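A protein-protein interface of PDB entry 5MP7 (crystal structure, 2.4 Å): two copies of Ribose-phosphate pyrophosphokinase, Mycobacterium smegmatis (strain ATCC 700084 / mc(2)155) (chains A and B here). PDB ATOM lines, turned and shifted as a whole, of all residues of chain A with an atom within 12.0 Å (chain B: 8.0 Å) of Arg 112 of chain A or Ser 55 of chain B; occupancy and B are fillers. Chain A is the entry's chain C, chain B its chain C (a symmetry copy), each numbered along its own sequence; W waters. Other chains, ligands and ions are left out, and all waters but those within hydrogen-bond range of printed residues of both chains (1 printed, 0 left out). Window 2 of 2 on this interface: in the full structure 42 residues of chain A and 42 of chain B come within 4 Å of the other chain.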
ATOM      1  N   GLN A 105     -11.734  13.283  12.294  1.00  0.00           N
ATOM      2  CA  GLN A 105     -12.387  14.419  12.922  1.00  0.00           C
ATOM      3  C   GLN A 105     -11.896  14.589  14.378  1.00  0.00           C
ATOM      4  O   GLN A 105     -12.653  14.379  15.316  1.00  0.00           O
ATOM      5  CB  GLN A 105     -13.901  14.224  12.832  1.00  0.00           C
ATOM      6  CG  GLN A 105     -14.709  15.464  13.195  1.00  0.00           C
ATOM      7  CD  GLN A 105     -14.550  16.614  12.209  1.00  0.00           C
ATOM      8  OE1 GLN A 105     -14.600  16.425  11.008  1.00  0.00           O
ATOM      9  NE2 GLN A 105     -14.349  17.807  12.728  1.00  0.00           N
ATOM     10  N   ASP A 106     -10.631  14.990  14.536  1.00  0.00           N
ATOM     11  CA  ASP A 106      -9.979  15.147  15.858  1.00  0.00           C
ATOM     12  C   ASP A 106      -9.706  16.606  16.244  1.00  0.00           C
ATOM     13  O   ASP A 106      -8.996  16.885  17.216  1.00  0.00           O
ATOM     14  CB  ASP A 106      -8.667  14.364  15.903  1.00  0.00           C
ATOM     15  CG  ASP A 106      -7.715  14.709  14.733  1.00  0.00           C
ATOM     16  OD1 ASP A 106      -7.988  15.623  13.904  1.00  0.00           O
ATOM     17  OD2 ASP A 106      -6.694  14.009  14.611  1.00  0.00           O
ATOM     18  N   LYS A 107     -10.297  17.527  15.487  1.00  0.00           N
ATOM     19  CA  LYS A 107     -10.243  18.948  15.771  1.00  0.00           C
ATOM     20  C   LYS A 107     -11.322  19.639  14.948  1.00  0.00           C
ATOM     21  O   LYS A 107     -11.895  19.029  14.065  1.00  0.00           O
ATOM     22  CB  LYS A 107      -8.897  19.527  15.375  1.00  0.00           C
ATOM     23  CG  LYS A 107      -8.655  19.490  13.887  1.00  0.00           C
ATOM     24  CD  LYS A 107      -7.209  19.774  13.700  1.00  0.00           C
ATOM     25  CE  LYS A 107      -6.952  20.299  12.338  1.00  0.00           C
ATOM     26  NZ  LYS A 107      -5.486  20.398  12.152  1.00  0.00           N
ATOM     27  N   LYS A 108     -11.535  20.935  15.196  1.00  0.00           N
ATOM     28  CA  LYS A 108     -12.610  21.670  14.561  1.00  0.00           C
ATOM     29  C   LYS A 108     -12.373  22.186  13.159  1.00  0.00           C
ATOM     30  O   LYS A 108     -13.343  22.508  12.489  1.00  0.00           O
ATOM     31  CB  LYS A 108     -13.107  22.793  15.471  1.00  0.00           C
ATOM     32  CG  LYS A 108     -14.022  22.253  16.547  1.00  0.00           C
ATOM     33  CD  LYS A 108     -14.235  23.192  17.702  1.00  0.00           C
ATOM     34  CE  LYS A 108     -15.474  24.036  17.563  1.00  0.00           C
ATOM     35  NZ  LYS A 108     -15.496  25.084  18.635  1.00  0.00           N
ATOM     36  N   HIS A 109     -11.128  22.273  12.698  1.00  0.00           N
ATOM     37  CA  HIS A 109     -10.820  22.780  11.317  1.00  0.00           C
ATOM     38  C   HIS A 109     -11.336  24.178  11.055  1.00  0.00           C
ATOM     39  O   HIS A 109     -11.826  24.441   9.987  1.00  0.00           O
ATOM     40  CB  HIS A 109     -11.379  21.866  10.231  1.00  0.00           C
ATOM     41  CG  HIS A 109     -10.961  20.443  10.372  1.00  0.00           C
ATOM     42  ND1 HIS A 109      -9.718  19.991   9.990  1.00  0.00           N
ATOM     43  CD2 HIS A 109     -11.616  19.374  10.883  1.00  0.00           C
ATOM     44  CE1 HIS A 109      -9.625  18.698  10.254  1.00  0.00           C
ATOM     45  NE2 HIS A 109     -10.763  18.299  10.798  1.00  0.00           N
ATOM     46  N   ARG A 110     -11.245  25.047  12.061  1.00  0.00           N
ATOM     47  CA  ARG A 110     -11.868  26.392  12.071  1.00  0.00           C
ATOM     48  C   ARG A 110     -13.416  26.410  12.055  1.00  0.00           C
ATOM     49  O   ARG A 110     -14.017  27.043  11.194  1.00  0.00           O
ATOM     50  CB  ARG A 110     -11.292  27.271  10.965  1.00  0.00           C
ATOM     51  CG  ARG A 110      -9.814  27.505  11.118  1.00  0.00           C
ATOM     52  CD  ARG A 110      -9.452  28.566  12.099  1.00  0.00           C
ATOM     53  NE  ARG A 110      -8.089  29.050  11.868  1.00  0.00           N
ATOM     54  CZ  ARG A 110      -7.586  30.182  12.365  1.00  0.00           C
ATOM     55  NH1 ARG A 110      -8.313  30.970  13.169  1.00  0.00           N
ATOM     56  NH2 ARG A 110      -6.333  30.521  12.061  1.00  0.00           N
ATOM     57  N   GLY A 111     -14.012  25.663  13.011  1.00  0.00           N
ATOM     58  CA  GLY A 111     -15.461  25.735  13.455  1.00  0.00           C
ATOM     59  C   GLY A 111     -16.424  25.390  12.342  1.00  0.00           C
ATOM     60  O   GLY A 111     -15.948  25.071  11.260  1.00  0.00           O
ATOM     61  N   ARG A 112     -17.752  25.334  12.534  1.00  0.00           N
ATOM     62  CA  ARG A 112     -18.460  24.997  13.746  1.00  0.00           C
ATOM     63  C   ARG A 112     -18.786  23.522  13.693  1.00  0.00           C
ATOM     64  O   ARG A 112     -19.863  23.110  13.263  1.00  0.00           O
ATOM     65  CB  ARG A 112     -19.755  25.767  13.808  1.00  0.00           C
ATOM     66  CG  ARG A 112     -19.514  27.253  13.676  1.00  0.00           C
ATOM     67  CD  ARG A 112     -20.663  28.118  14.084  1.00  0.00           C
ATOM     68  NE  ARG A 112     -20.434  29.474  13.639  1.00  0.00           N
ATOM     69  CZ  ARG A 112     -20.532  29.915  12.381  1.00  0.00           C
ATOM     70  NH1 ARG A 112     -20.876  29.116  11.363  1.00  0.00           N
ATOM     71  NH2 ARG A 112     -20.290  31.196  12.142  1.00  0.00           N
ATOM     72  N   GLU A 113     -17.848  22.734  14.168  1.00  0.00           N
ATOM     73  CA  GLU A 113     -17.820  21.329  13.906  1.00  0.00           C
ATOM     74  C   GLU A 113     -17.724  20.581  15.216  1.00  0.00           C
ATOM     75  O   GLU A 113     -17.436  21.169  16.256  1.00  0.00           O
ATOM     76  CB  GLU A 113     -16.597  21.024  13.064  1.00  0.00           C
ATOM     77  CG  GLU A 113     -16.726  21.593  11.672  1.00  0.00           C
ATOM     78  CD  GLU A 113     -15.483  21.380  10.781  1.00  0.00           C
ATOM     79  OE1 GLU A 113     -14.949  20.240  10.730  1.00  0.00           O
ATOM     80  OE2 GLU A 113     -14.985  22.369  10.139  1.00  0.00           O
ATOM     81  N   PRO A 114     -18.013  19.290  15.168  1.00  0.00           N
ATOM     82  CA  PRO A 114     -17.818  18.437  16.307  1.00  0.00           C
ATOM     83  C   PRO A 114     -16.384  17.937  16.360  1.00  0.00           C
ATOM     84  O   PRO A 114     -15.659  17.999  15.366  1.00  0.00           O
ATOM     85  CB  PRO A 114     -18.724  17.277  15.998  1.00  0.00           C
ATOM     86  CG  PRO A 114     -18.665  17.179  14.511  1.00  0.00           C
ATOM     87  CD  PRO A 114     -18.582  18.570  14.022  1.00  0.00           C
ATOM     88  N   ILE A 115     -15.980  17.456  17.518  1.00  0.00           N
ATOM     89  CA  ILE A 115     -14.762  16.691  17.623  1.00  0.00           C
ATOM     90  C   ILE A 115     -15.175  15.244  17.814  1.00  0.00           C
ATOM     91  O   ILE A 115     -15.275  14.743  18.910  1.00  0.00           O
ATOM     92  CB  ILE A 115     -13.838  17.194  18.737  1.00  0.00           C
ATOM     93  CG1 ILE A 115     -13.573  18.675  18.522  1.00  0.00           C
ATOM     94  CG2 ILE A 115     -12.521  16.431  18.638  1.00  0.00           C
ATOM     95  CD1 ILE A 115     -12.640  19.332  19.520  1.00  0.00           C
ATOM     96  N   SER A 116     -15.494  14.616  16.712  1.00  0.00           N
ATOM     97  CA  SER A 116     -16.101  13.288  16.724  1.00  0.00           C
ATOM     98  C   SER A 116     -15.230  12.208  17.295  1.00  0.00           C
ATOM     99  O   SER A 116     -15.747  11.258  17.882  1.00  0.00           O
ATOM    100  CB  SER A 116     -16.499  12.881  15.334  1.00  0.00           C
ATOM    101  OG  SER A 116     -17.583  13.676  14.947  1.00  0.00           O
ATOM    102  N   ASN B  11     -32.907  32.533  22.348  1.00  0.00           N
ATOM    103  CA  ASN B  11     -32.984  32.399  20.923  1.00  0.00           C
ATOM    104  C   ASN B  11     -33.259  30.929  20.559  1.00  0.00           C
ATOM    105  O   ASN B  11     -32.470  30.034  20.879  1.00  0.00           O
ATOM    106  CB  ASN B  11     -31.668  32.905  20.347  1.00  0.00           C
ATOM    107  CG  ASN B  11     -31.527  32.595  18.869  1.00  0.00           C
ATOM    108  OD1 ASN B  11     -32.431  32.853  18.071  1.00  0.00           O
ATOM    109  ND2 ASN B  11     -30.360  32.096  18.483  1.00  0.00           N
ATOM    110  N   MET B  13     -33.453  27.786  18.209  1.00  0.00           N
ATOM    111  CA  MET B  13     -32.903  27.258  16.967  1.00  0.00           C
ATOM    112  C   MET B  13     -33.229  25.803  16.810  1.00  0.00           C
ATOM    113  O   MET B  13     -33.058  24.989  17.716  1.00  0.00           O
ATOM    114  CB  MET B  13     -31.392  27.451  16.917  1.00  0.00           C
ATOM    115  CG  MET B  13     -31.019  28.864  16.560  1.00  0.00           C
ATOM    116  SD  MET B  13     -29.245  29.109  16.553  1.00  0.00           S
ATOM    117  CE  MET B  13     -28.850  28.701  14.851  1.00  0.00           C
ATOM    118  N   PHE B  15     -32.632  22.327  14.676  1.00  0.00           N
ATOM    119  CA  PHE B  15     -31.688  21.584  13.879  1.00  0.00           C
ATOM    120  C   PHE B  15     -32.367  20.279  13.512  1.00  0.00           C
ATOM    121  O   PHE B  15     -33.154  19.752  14.259  1.00  0.00           O
ATOM    122  CB  PHE B  15     -30.449  21.276  14.688  1.00  0.00           C
ATOM    123  CG  PHE B  15     -29.773  22.492  15.193  1.00  0.00           C
ATOM    124  CD1 PHE B  15     -30.188  23.103  16.367  1.00  0.00           C
ATOM    125  CD2 PHE B  15     -28.748  23.060  14.479  1.00  0.00           C
ATOM    126  CE1 PHE B  15     -29.577  24.285  16.791  1.00  0.00           C
ATOM    127  CE2 PHE B  15     -28.148  24.220  14.893  1.00  0.00           C
ATOM    128  CZ  PHE B  15     -28.550  24.840  16.037  1.00  0.00           C
ATOM    129  N   THR B  36     -32.052  25.461  10.853  1.00  0.00           N
ATOM    130  CA  THR B  36     -30.704  26.041  10.787  1.00  0.00           C
ATOM    131  C   THR B  36     -29.869  25.348   9.703  1.00  0.00           C
ATOM    132  O   THR B  36     -29.872  24.119   9.603  1.00  0.00           O
ATOM    133  CB  THR B  36     -30.001  25.880  12.145  1.00  0.00           C
ATOM    134  OG1 THR B  36     -30.798  26.520  13.137  1.00  0.00           O
ATOM    135  CG2 THR B  36     -28.654  26.516  12.148  1.00  0.00           C
ATOM    136  N   ALA B  37     -29.125  26.151   8.943  1.00  0.00           N
ATOM    137  CA  ALA B  37     -28.332  25.653   7.830  1.00  0.00           C
ATOM    138  C   ALA B  37     -27.191  24.820   8.340  1.00  0.00           C
ATOM    139  O   ALA B  37     -26.521  25.190   9.287  1.00  0.00           O
ATOM    140  CB  ALA B  37     -27.796  26.814   6.996  1.00  0.00           C
ATOM    141  N   GLN B  38     -26.986  23.683   7.711  1.00  0.00           N
ATOM    142  CA  GLN B  38     -25.873  22.854   8.037  1.00  0.00           C
ATOM    143  C   GLN B  38     -25.495  21.914   6.931  1.00  0.00           C
ATOM    144  O   GLN B  38     -26.298  21.564   6.101  1.00  0.00           O
ATOM    145  CB  GLN B  38     -26.194  22.042   9.249  1.00  0.00           C
ATOM    146  CG  GLN B  38     -27.338  21.079   9.085  1.00  0.00           C
ATOM    147  CD  GLN B  38     -27.360  20.131  10.263  1.00  0.00           C
ATOM    148  OE1 GLN B  38     -26.493  19.280  10.428  1.00  0.00           O
ATOM    149  NE2 GLN B  38     -28.322  20.328  11.119  1.00  0.00           N
ATOM    150  N   THR B  39     -24.221  21.570   6.897  1.00  0.00           N
ATOM    151  CA  THR B  39     -23.693  20.631   5.930  1.00  0.00           C
ATOM    152  C   THR B  39     -23.761  19.289   6.640  1.00  0.00           C
ATOM    153  O   THR B  39     -23.198  19.172   7.705  1.00  0.00           O
ATOM    154  CB  THR B  39     -22.229  20.977   5.593  1.00  0.00           C
ATOM    155  OG1 THR B  39     -22.124  22.350   5.203  1.00  0.00           O
ATOM    156  CG2 THR B  39     -21.719  20.089   4.485  1.00  0.00           C
ATOM    157  N   PHE B  49     -20.146  13.643   8.475  1.00  0.00           N
ATOM    158  CA  PHE B  49     -19.546  14.931   8.642  1.00  0.00           C
ATOM    159  C   PHE B  49     -20.642  15.938   8.888  1.00  0.00           C
ATOM    160  O   PHE B  49     -21.612  15.984   8.147  1.00  0.00           O
ATOM    161  CB  PHE B  49     -18.834  15.322   7.368  1.00  0.00           C
ATOM    162  CG  PHE B  49     -18.239  16.696   7.422  1.00  0.00           C
ATOM    163  CD1 PHE B  49     -17.014  16.915   8.058  1.00  0.00           C
ATOM    164  CD2 PHE B  49     -18.895  17.786   6.854  1.00  0.00           C
ATOM    165  CE1 PHE B  49     -16.444  18.191   8.125  1.00  0.00           C
ATOM    166  CE2 PHE B  49     -18.330  19.076   6.920  1.00  0.00           C
ATOM    167  CZ  PHE B  49     -17.098  19.267   7.552  1.00  0.00           C
ATOM    168  N   VAL B  50     -20.470  16.785   9.887  1.00  0.00           N
ATOM    169  CA  VAL B  50     -21.492  17.741  10.250  1.00  0.00           C
ATOM    170  C   VAL B  50     -20.826  19.069  10.445  1.00  0.00           C
ATOM    171  O   VAL B  50     -19.840  19.151  11.126  1.00  0.00           O
ATOM    172  CB  VAL B  50     -22.256  17.263  11.538  1.00  0.00           C
ATOM    173  CG1 VAL B  50     -22.788  18.422  12.382  1.00  0.00           C
ATOM    174  CG2 VAL B  50     -23.435  16.357  11.180  1.00  0.00           C
ATOM    175  N   ARG B  51     -21.418  20.127   9.928  1.00  0.00           N
ATOM    176  CA  ARG B  51     -20.946  21.481  10.217  1.00  0.00           C
ATOM    177  C   ARG B  51     -22.088  22.500  10.189  1.00  0.00           C
ATOM    178  O   ARG B  51     -22.890  22.475   9.271  1.00  0.00           O
ATOM    179  CB  ARG B  51     -19.916  21.886   9.186  1.00  0.00           C
ATOM    180  CG  ARG B  51     -19.240  23.212   9.533  1.00  0.00           C
ATOM    181  CD  ARG B  51     -18.208  23.552   8.503  1.00  0.00           C
ATOM    182  NE  ARG B  51     -18.864  23.554   7.207  1.00  0.00           N
ATOM    183  CZ  ARG B  51     -18.326  23.161   6.056  1.00  0.00           C
ATOM    184  NH1 ARG B  51     -17.062  22.693   5.988  1.00  0.00           N
ATOM    185  NH2 ARG B  51     -19.082  23.226   4.949  1.00  0.00           N
ATOM    186  N   PHE B  52     -22.153  23.394  11.171  1.00  0.00           N
ATOM    187  CA  PHE B  52     -23.224  24.385  11.207  1.00  0.00           C
ATOM    188  C   PHE B  52     -22.794  25.606  10.437  1.00  0.00           C
ATOM    189  O   PHE B  52     -21.682  26.056  10.567  1.00  0.00           O
ATOM    190  CB  PHE B  52     -23.614  24.739  12.617  1.00  0.00           C
ATOM    191  CG  PHE B  52     -24.127  23.585  13.392  1.00  0.00           C
ATOM    192  CD1 PHE B  52     -25.215  22.860  12.935  1.00  0.00           C
ATOM    193  CD2 PHE B  52     -23.535  23.211  14.585  1.00  0.00           C
ATOM    194  CE1 PHE B  52     -25.692  21.754  13.633  1.00  0.00           C
ATOM    195  CE2 PHE B  52     -24.023  22.119  15.310  1.00  0.00           C
ATOM    196  CZ  PHE B  52     -25.084  21.371  14.824  1.00  0.00           C
ATOM    197  N   ASP B  53     -23.681  26.105   9.594  1.00  0.00           N
ATOM    198  CA  ASP B  53     -23.321  27.171   8.681  1.00  0.00           C
ATOM    199  C   ASP B  53     -23.796  28.554   9.114  1.00  0.00           C
ATOM    200  O   ASP B  53     -23.776  29.489   8.324  1.00  0.00           O
ATOM    201  CB  ASP B  53     -23.766  26.790   7.282  1.00  0.00           C
ATOM    202  CG  ASP B  53     -22.951  25.595   6.727  1.00  0.00           C
ATOM    203  OD1 ASP B  53     -21.767  25.421   7.037  1.00  0.00           O
ATOM    204  OD2 ASP B  53     -23.514  24.795   5.976  1.00  0.00           O
ATOM    205  N   GLU B  54     -24.236  28.668  10.361  1.00  0.00           N
ATOM    206  CA  GLU B  54     -24.502  29.947  10.976  1.00  0.00           C
ATOM    207  C   GLU B  54     -24.204  29.773  12.449  1.00  0.00           C
ATOM    208  O   GLU B  54     -23.968  28.635  12.909  1.00  0.00           O
ATOM    209  CB  GLU B  54     -25.950  30.422  10.746  1.00  0.00           C
ATOM    210  CG  GLU B  54     -27.033  29.343  10.866  1.00  0.00           C
ATOM    211  CD  GLU B  54     -28.460  29.859  10.612  1.00  0.00           C
ATOM    212  OE1 GLU B  54     -28.928  30.701  11.409  1.00  0.00           O
ATOM    213  OE2 GLU B  54     -29.117  29.382   9.646  1.00  0.00           O
ATOM    214  N   SER B  55     -24.166  30.883  13.184  1.00  0.00           N
ATOM    215  CA  SER B  55     -23.756  30.829  14.586  1.00  0.00           C
ATOM    216  C   SER B  55     -24.801  30.117  15.432  1.00  0.00           C
ATOM    217  O   SER B  55     -25.976  30.275  15.204  1.00  0.00           O
ATOM    218  CB  SER B  55     -23.493  32.229  15.164  1.00  0.00           C
ATOM    219  OG  SER B  55     -22.747  32.116  16.381  1.00  0.00           O
ATOM    220  N   VAL B  56     -24.340  29.334  16.397  1.00  0.00           N
ATOM    221  CA  VAL B  56     -25.212  28.651  17.340  1.00  0.00           C
ATOM    222  C   VAL B  56     -24.944  29.024  18.798  1.00  0.00           C
ATOM    223  O   VAL B  56     -25.580  28.529  19.699  1.00  0.00           O
ATOM    224  CB  VAL B  56     -25.092  27.130  17.172  1.00  0.00           C
ATOM    225  CG1 VAL B  56     -25.426  26.742  15.757  1.00  0.00           C
ATOM    226  CG2 VAL B  56     -23.704  26.625  17.515  1.00  0.00           C
ATOM    227  N   ARG B  57     -23.975  29.894  19.026  1.00  0.00           N
ATOM    228  CA  ARG B  57     -23.581  30.328  20.341  1.00  0.00           C
ATOM    229  C   ARG B  57     -24.780  30.940  21.086  1.00  0.00           C
ATOM    230  O   ARG B  57     -25.498  31.757  20.539  1.00  0.00           O
ATOM    231  CB  ARG B  57     -22.398  31.268  20.139  1.00  0.00           C
ATOM    232  CG  ARG B  57     -21.770  31.875  21.345  1.00  0.00           C
ATOM    233  CD  ARG B  57     -20.647  32.821  20.827  1.00  0.00           C
ATOM    234  NE  ARG B  57     -19.528  32.142  20.131  1.00  0.00           N
ATOM    235  CZ  ARG B  57     -18.598  31.445  20.776  1.00  0.00           C
ATOM    236  NH1 ARG B  57     -18.639  31.320  22.106  1.00  0.00           N
ATOM    237  NH2 ARG B  57     -17.626  30.871  20.113  1.00  0.00           N
ATOM    238  N   GLY B  58     -25.023  30.457  22.306  1.00  0.00           N
ATOM    239  CA  GLY B  58     -26.045  30.976  23.193  1.00  0.00           C
ATOM    240  C   GLY B  58     -27.493  30.585  22.930  1.00  0.00           C
ATOM    241  O   GLY B  58     -28.393  31.047  23.642  1.00  0.00           O
ATOM    242  N   CYS B  59     -27.732  29.696  21.976  1.00  0.00           N
ATOM    243  CA  CYS B  59     -29.096  29.317  21.577  1.00  0.00           C
ATOM    244  C   CYS B  59     -29.733  28.231  22.462  1.00  0.00           C
ATOM    245  O   CYS B  59     -29.054  27.481  23.160  1.00  0.00           O
ATOM    246  CB  CYS B  59     -29.105  28.838  20.103  1.00  0.00           C
ATOM    247  SG  CYS B  59     -28.442  27.159  19.830  1.00  0.00           S
ATOM    248  N   ILE B  80     -23.637  13.255  17.047  1.00  0.00           N
ATOM    249  CA  ILE B  80     -22.597  14.135  16.491  1.00  0.00           C
ATOM    250  C   ILE B  80     -23.064  15.578  16.500  1.00  0.00           C
ATOM    251  O   ILE B  80     -22.296  16.475  16.837  1.00  0.00           O
ATOM    252  CB  ILE B  80     -22.145  13.652  15.090  1.00  0.00           C
ATOM    253  CG1 ILE B  80     -21.272  12.417  15.253  1.00  0.00           C
ATOM    254  CG2 ILE B  80     -21.335  14.691  14.338  1.00  0.00           C
ATOM    255  CD1 ILE B  80     -21.207  11.559  14.006  1.00  0.00           C
ATOM    256  N   MET B  81     -24.310  15.819  16.138  1.00  0.00           N
ATOM    257  CA  MET B  81     -24.872  17.196  16.161  1.00  0.00           C
ATOM    258  C   MET B  81     -24.932  17.773  17.573  1.00  0.00           C
ATOM    259  O   MET B  81     -24.671  18.940  17.781  1.00  0.00           O
ATOM    260  CB  MET B  81     -26.285  17.221  15.550  1.00  0.00           C
ATOM    261  CG  MET B  81     -26.289  17.220  14.037  1.00  0.00           C
ATOM    262  SD  MET B  81     -27.881  16.863  13.231  1.00  0.00           S
ATOM    263  CE  MET B  81     -28.649  18.435  13.355  1.00  0.00           C
ATOM    264  N   ALA B  84     -21.401  18.856  18.546  1.00  0.00           N
ATOM    265  CA  ALA B  84     -21.048  20.084  17.924  1.00  0.00           C
ATOM    266  C   ALA B  84     -21.716  21.278  18.592  1.00  0.00           C
ATOM    267  O   ALA B  84     -21.111  22.328  18.750  1.00  0.00           O
ATOM    268  CB  ALA B  84     -21.421  20.024  16.471  1.00  0.00           C
ATOM    269  N   LEU B  85     -22.973  21.140  18.979  1.00  0.00           N
ATOM    270  CA  LEU B  85     -23.659  22.215  19.707  1.00  0.00           C
ATOM    271  C   LEU B  85     -23.039  22.425  21.081  1.00  0.00           C
ATOM    272  O   LEU B  85     -22.957  23.557  21.564  1.00  0.00           O
ATOM    273  CB  LEU B  85     -25.161  21.913  19.884  1.00  0.00           C
ATOM    274  CG  LEU B  85     -25.974  21.956  18.609  1.00  0.00           C
ATOM    275  CD1 LEU B  85     -27.302  21.266  18.819  1.00  0.00           C
ATOM    276  CD2 LEU B  85     -26.227  23.383  18.135  1.00  0.00           C
ATOM    277  N   ARG B  87     -19.873  21.971  21.858  1.00  0.00           N
ATOM    278  CA  ARG B  87     -18.605  22.678  21.616  1.00  0.00           C
ATOM    279  C   ARG B  87     -18.756  24.024  20.946  1.00  0.00           C
ATOM    280  O   ARG B  87     -17.805  24.806  20.944  1.00  0.00           O
ATOM    281  CB  ARG B  87     -17.659  21.827  20.793  1.00  0.00           C
ATOM    282  CG  ARG B  87     -17.278  20.612  21.582  1.00  0.00           C
ATOM    283  CD  ARG B  87     -16.270  19.788  20.875  1.00  0.00           C
ATOM    284  NE  ARG B  87     -16.478  18.424  21.289  1.00  0.00           N
ATOM    285  CZ  ARG B  87     -15.926  17.827  22.335  1.00  0.00           C
ATOM    286  NH1 ARG B  87     -15.032  18.442  23.125  1.00  0.00           N
ATOM    287  NH2 ARG B  87     -16.264  16.563  22.575  1.00  0.00           N
ATOM    288  N   GLY B  88     -19.932  24.293  20.375  1.00  0.00           N
ATOM    289  CA  GLY B  88     -20.245  25.595  19.846  1.00  0.00           C
ATOM    290  C   GLY B  88     -20.937  26.511  20.823  1.00  0.00           C
ATOM    291  O   GLY B  88     -21.495  27.515  20.406  1.00  0.00           O
ATOM    292  N   SER B  89     -20.946  26.173  22.114  1.00  0.00           N
ATOM    293  CA  SER B  89     -21.526  27.022  23.170  1.00  0.00           C
ATOM    294  C   SER B  89     -23.017  27.296  23.032  1.00  0.00           C
ATOM    295  O   SER B  89     -23.469  28.379  23.343  1.00  0.00           O
ATOM    296  CB  SER B  89     -20.777  28.357  23.307  1.00  0.00           C
ATOM    297  OG  SER B  89     -19.422  28.118  23.654  1.00  0.00           O
HETATM  298  O   HOH W   1     -18.763  23.412  17.268  1.00  0.00           O
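No position is printed for both chains.
Of the 17 pairs that touch across the chains among the printed residues, none has its exchanged pair printed and touching as well.
NH1 of Arg 112 of chain A is in hydrogen-bond range of O of Glu 54 of chain B (3.5 Å).
The backbone NH (N) of Phe 52 of chain B sits at hydrogen-bond distance from the backbone carbonyl oxygen (O) of Arg 112 of chain A.
The backbone carbonyl oxygen (O) of Arg 87 of chain B sits at hydrogen-bond distance from the side-chain amino group (NZ) of Lys 108 of chain A, 3.3 Å away.
Of the 12 printed residues of chain A, 8 touch a printed residue of chain B.
Hydrophobic or aromatic side chains of chain A within 4 Å of the printed part of chain B: Pro 114 and Ile 115.
Hydrophobic or aromatic side chains of chain B that line the printed part of chain A: Phe 49, Phe 52, Ile 80 and Ala 84.
Among the printed residues, no Asp or Glu carboxylate lies within 4 Å of a Lys or Arg side-chain nitrogen of the other chain.
The backbone NH (N) of Ala 37 of chain B is in hydrogen-bond range of the side-chain carboxylate (OE2) of Glu 54 of chain B (3.3 Å).
N of Thr 39 of chain B is in hydrogen-bond range of O of Arg 51 of chain B (2.9 Å).
The side-chain carboxylate of Glu 113 of chain A is in hydrogen-bond range of the side-chain amide nitrogen of Gln 105 of chain A, 3.2 Å away.
The backbone carbonyl oxygen (O) of Gln 105 of chain A sits at hydrogen-bond distance from the backbone NH (N) of Ser 116 of chain A (3.2 Å).
The guanidinium group of Arg 51 of chain B lies within salt-bridge range of the side-chain carboxylate of Asp 53 of chain B (3.5 Å).
The side-chain amide nitrogen of Gln 105 of chain A is in hydrogen-bond range of the backbone carbonyl oxygen of Lys 107 of chain A, 3.1 Å away.
Water W1 lies within hydrogen-bond range of the backbone carbonyl oxygen of Glu 113 of chain A (2.8 Å), the backbone carbonyl oxygen of Ala 84 of chain B (3.0 Å) and the backbone NH of Gly 88 of chain B (3.4 Å).
O of Gly 111 of chain A touches CD of Arg 51 of chain B, 3.9 Å away.
Arg 112 of chain A touches Asp 53 of chain B.
NE of Arg 112 of chain A touches CA of Ser 55 of chain B, at 3.7 Å.
OE1 of Glu 113 of chain A touches CE1 of Phe 49 of chain B, 3.6 Å away.
CG of Glu 113 of chain A touches O of Val 50 of chain B, at 3.99 Å.
Arg 51 of chain B touches Glu 113 of chain A.
C of Glu 113 of chain A touches CB of Ala 84 of chain B, at 3.9 Å.
Pro 114 of chain A touches Ile 80 of chain B.
Pro 114 of chain A touches Ala 84 of chain B (N to CB, 3.7 Å).
Arg 87 of chain B touches Ile 115 of chain A.
Gly 111 of chain A touches just one residue of chain B: Arg 51.
Printed residues of chain B within 4 Å of Arg 112 of chain A: Arg 51 (3.6 Å), Phe 52 (3.1 Å), Asp 53 (3.7 Å), Glu 54 (3.5 Å) and Ser 55 (3.7 Å).
Printed residues of chain A within 4 Å of Phe 49 of chain B: Gln 105 and Glu 113.
Printed residues of chain A within 4 Å of Val 50 of chain B: Glu 113 (3.99 Å) and Pro 114 (3.2 Å).
Of chain A, only Arg 112 comes within 4 Å of Glu 54 of chain B.
Of the printed residues of chain A, Ser 55 of chain B touches Arg 112 (3.7 Å).
No residue of chain A comes within 4 Å of Arg 57 of chain B.
Ala 84 of chain B touches just these residues of chain A: Glu 113 and Pro 114.
Printed residues of chain A within 4 Å of Arg 87 of chain B: Lys 108 and Ile 115.
The nearest printed residue of chain B that does not touch Arg 112 of chain A is Val 50 of chain B (4.5 Å).
The nearest residue of chain A that does not touch Ser 55 of chain B is Gly 111 of chain A (9.4 Å).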
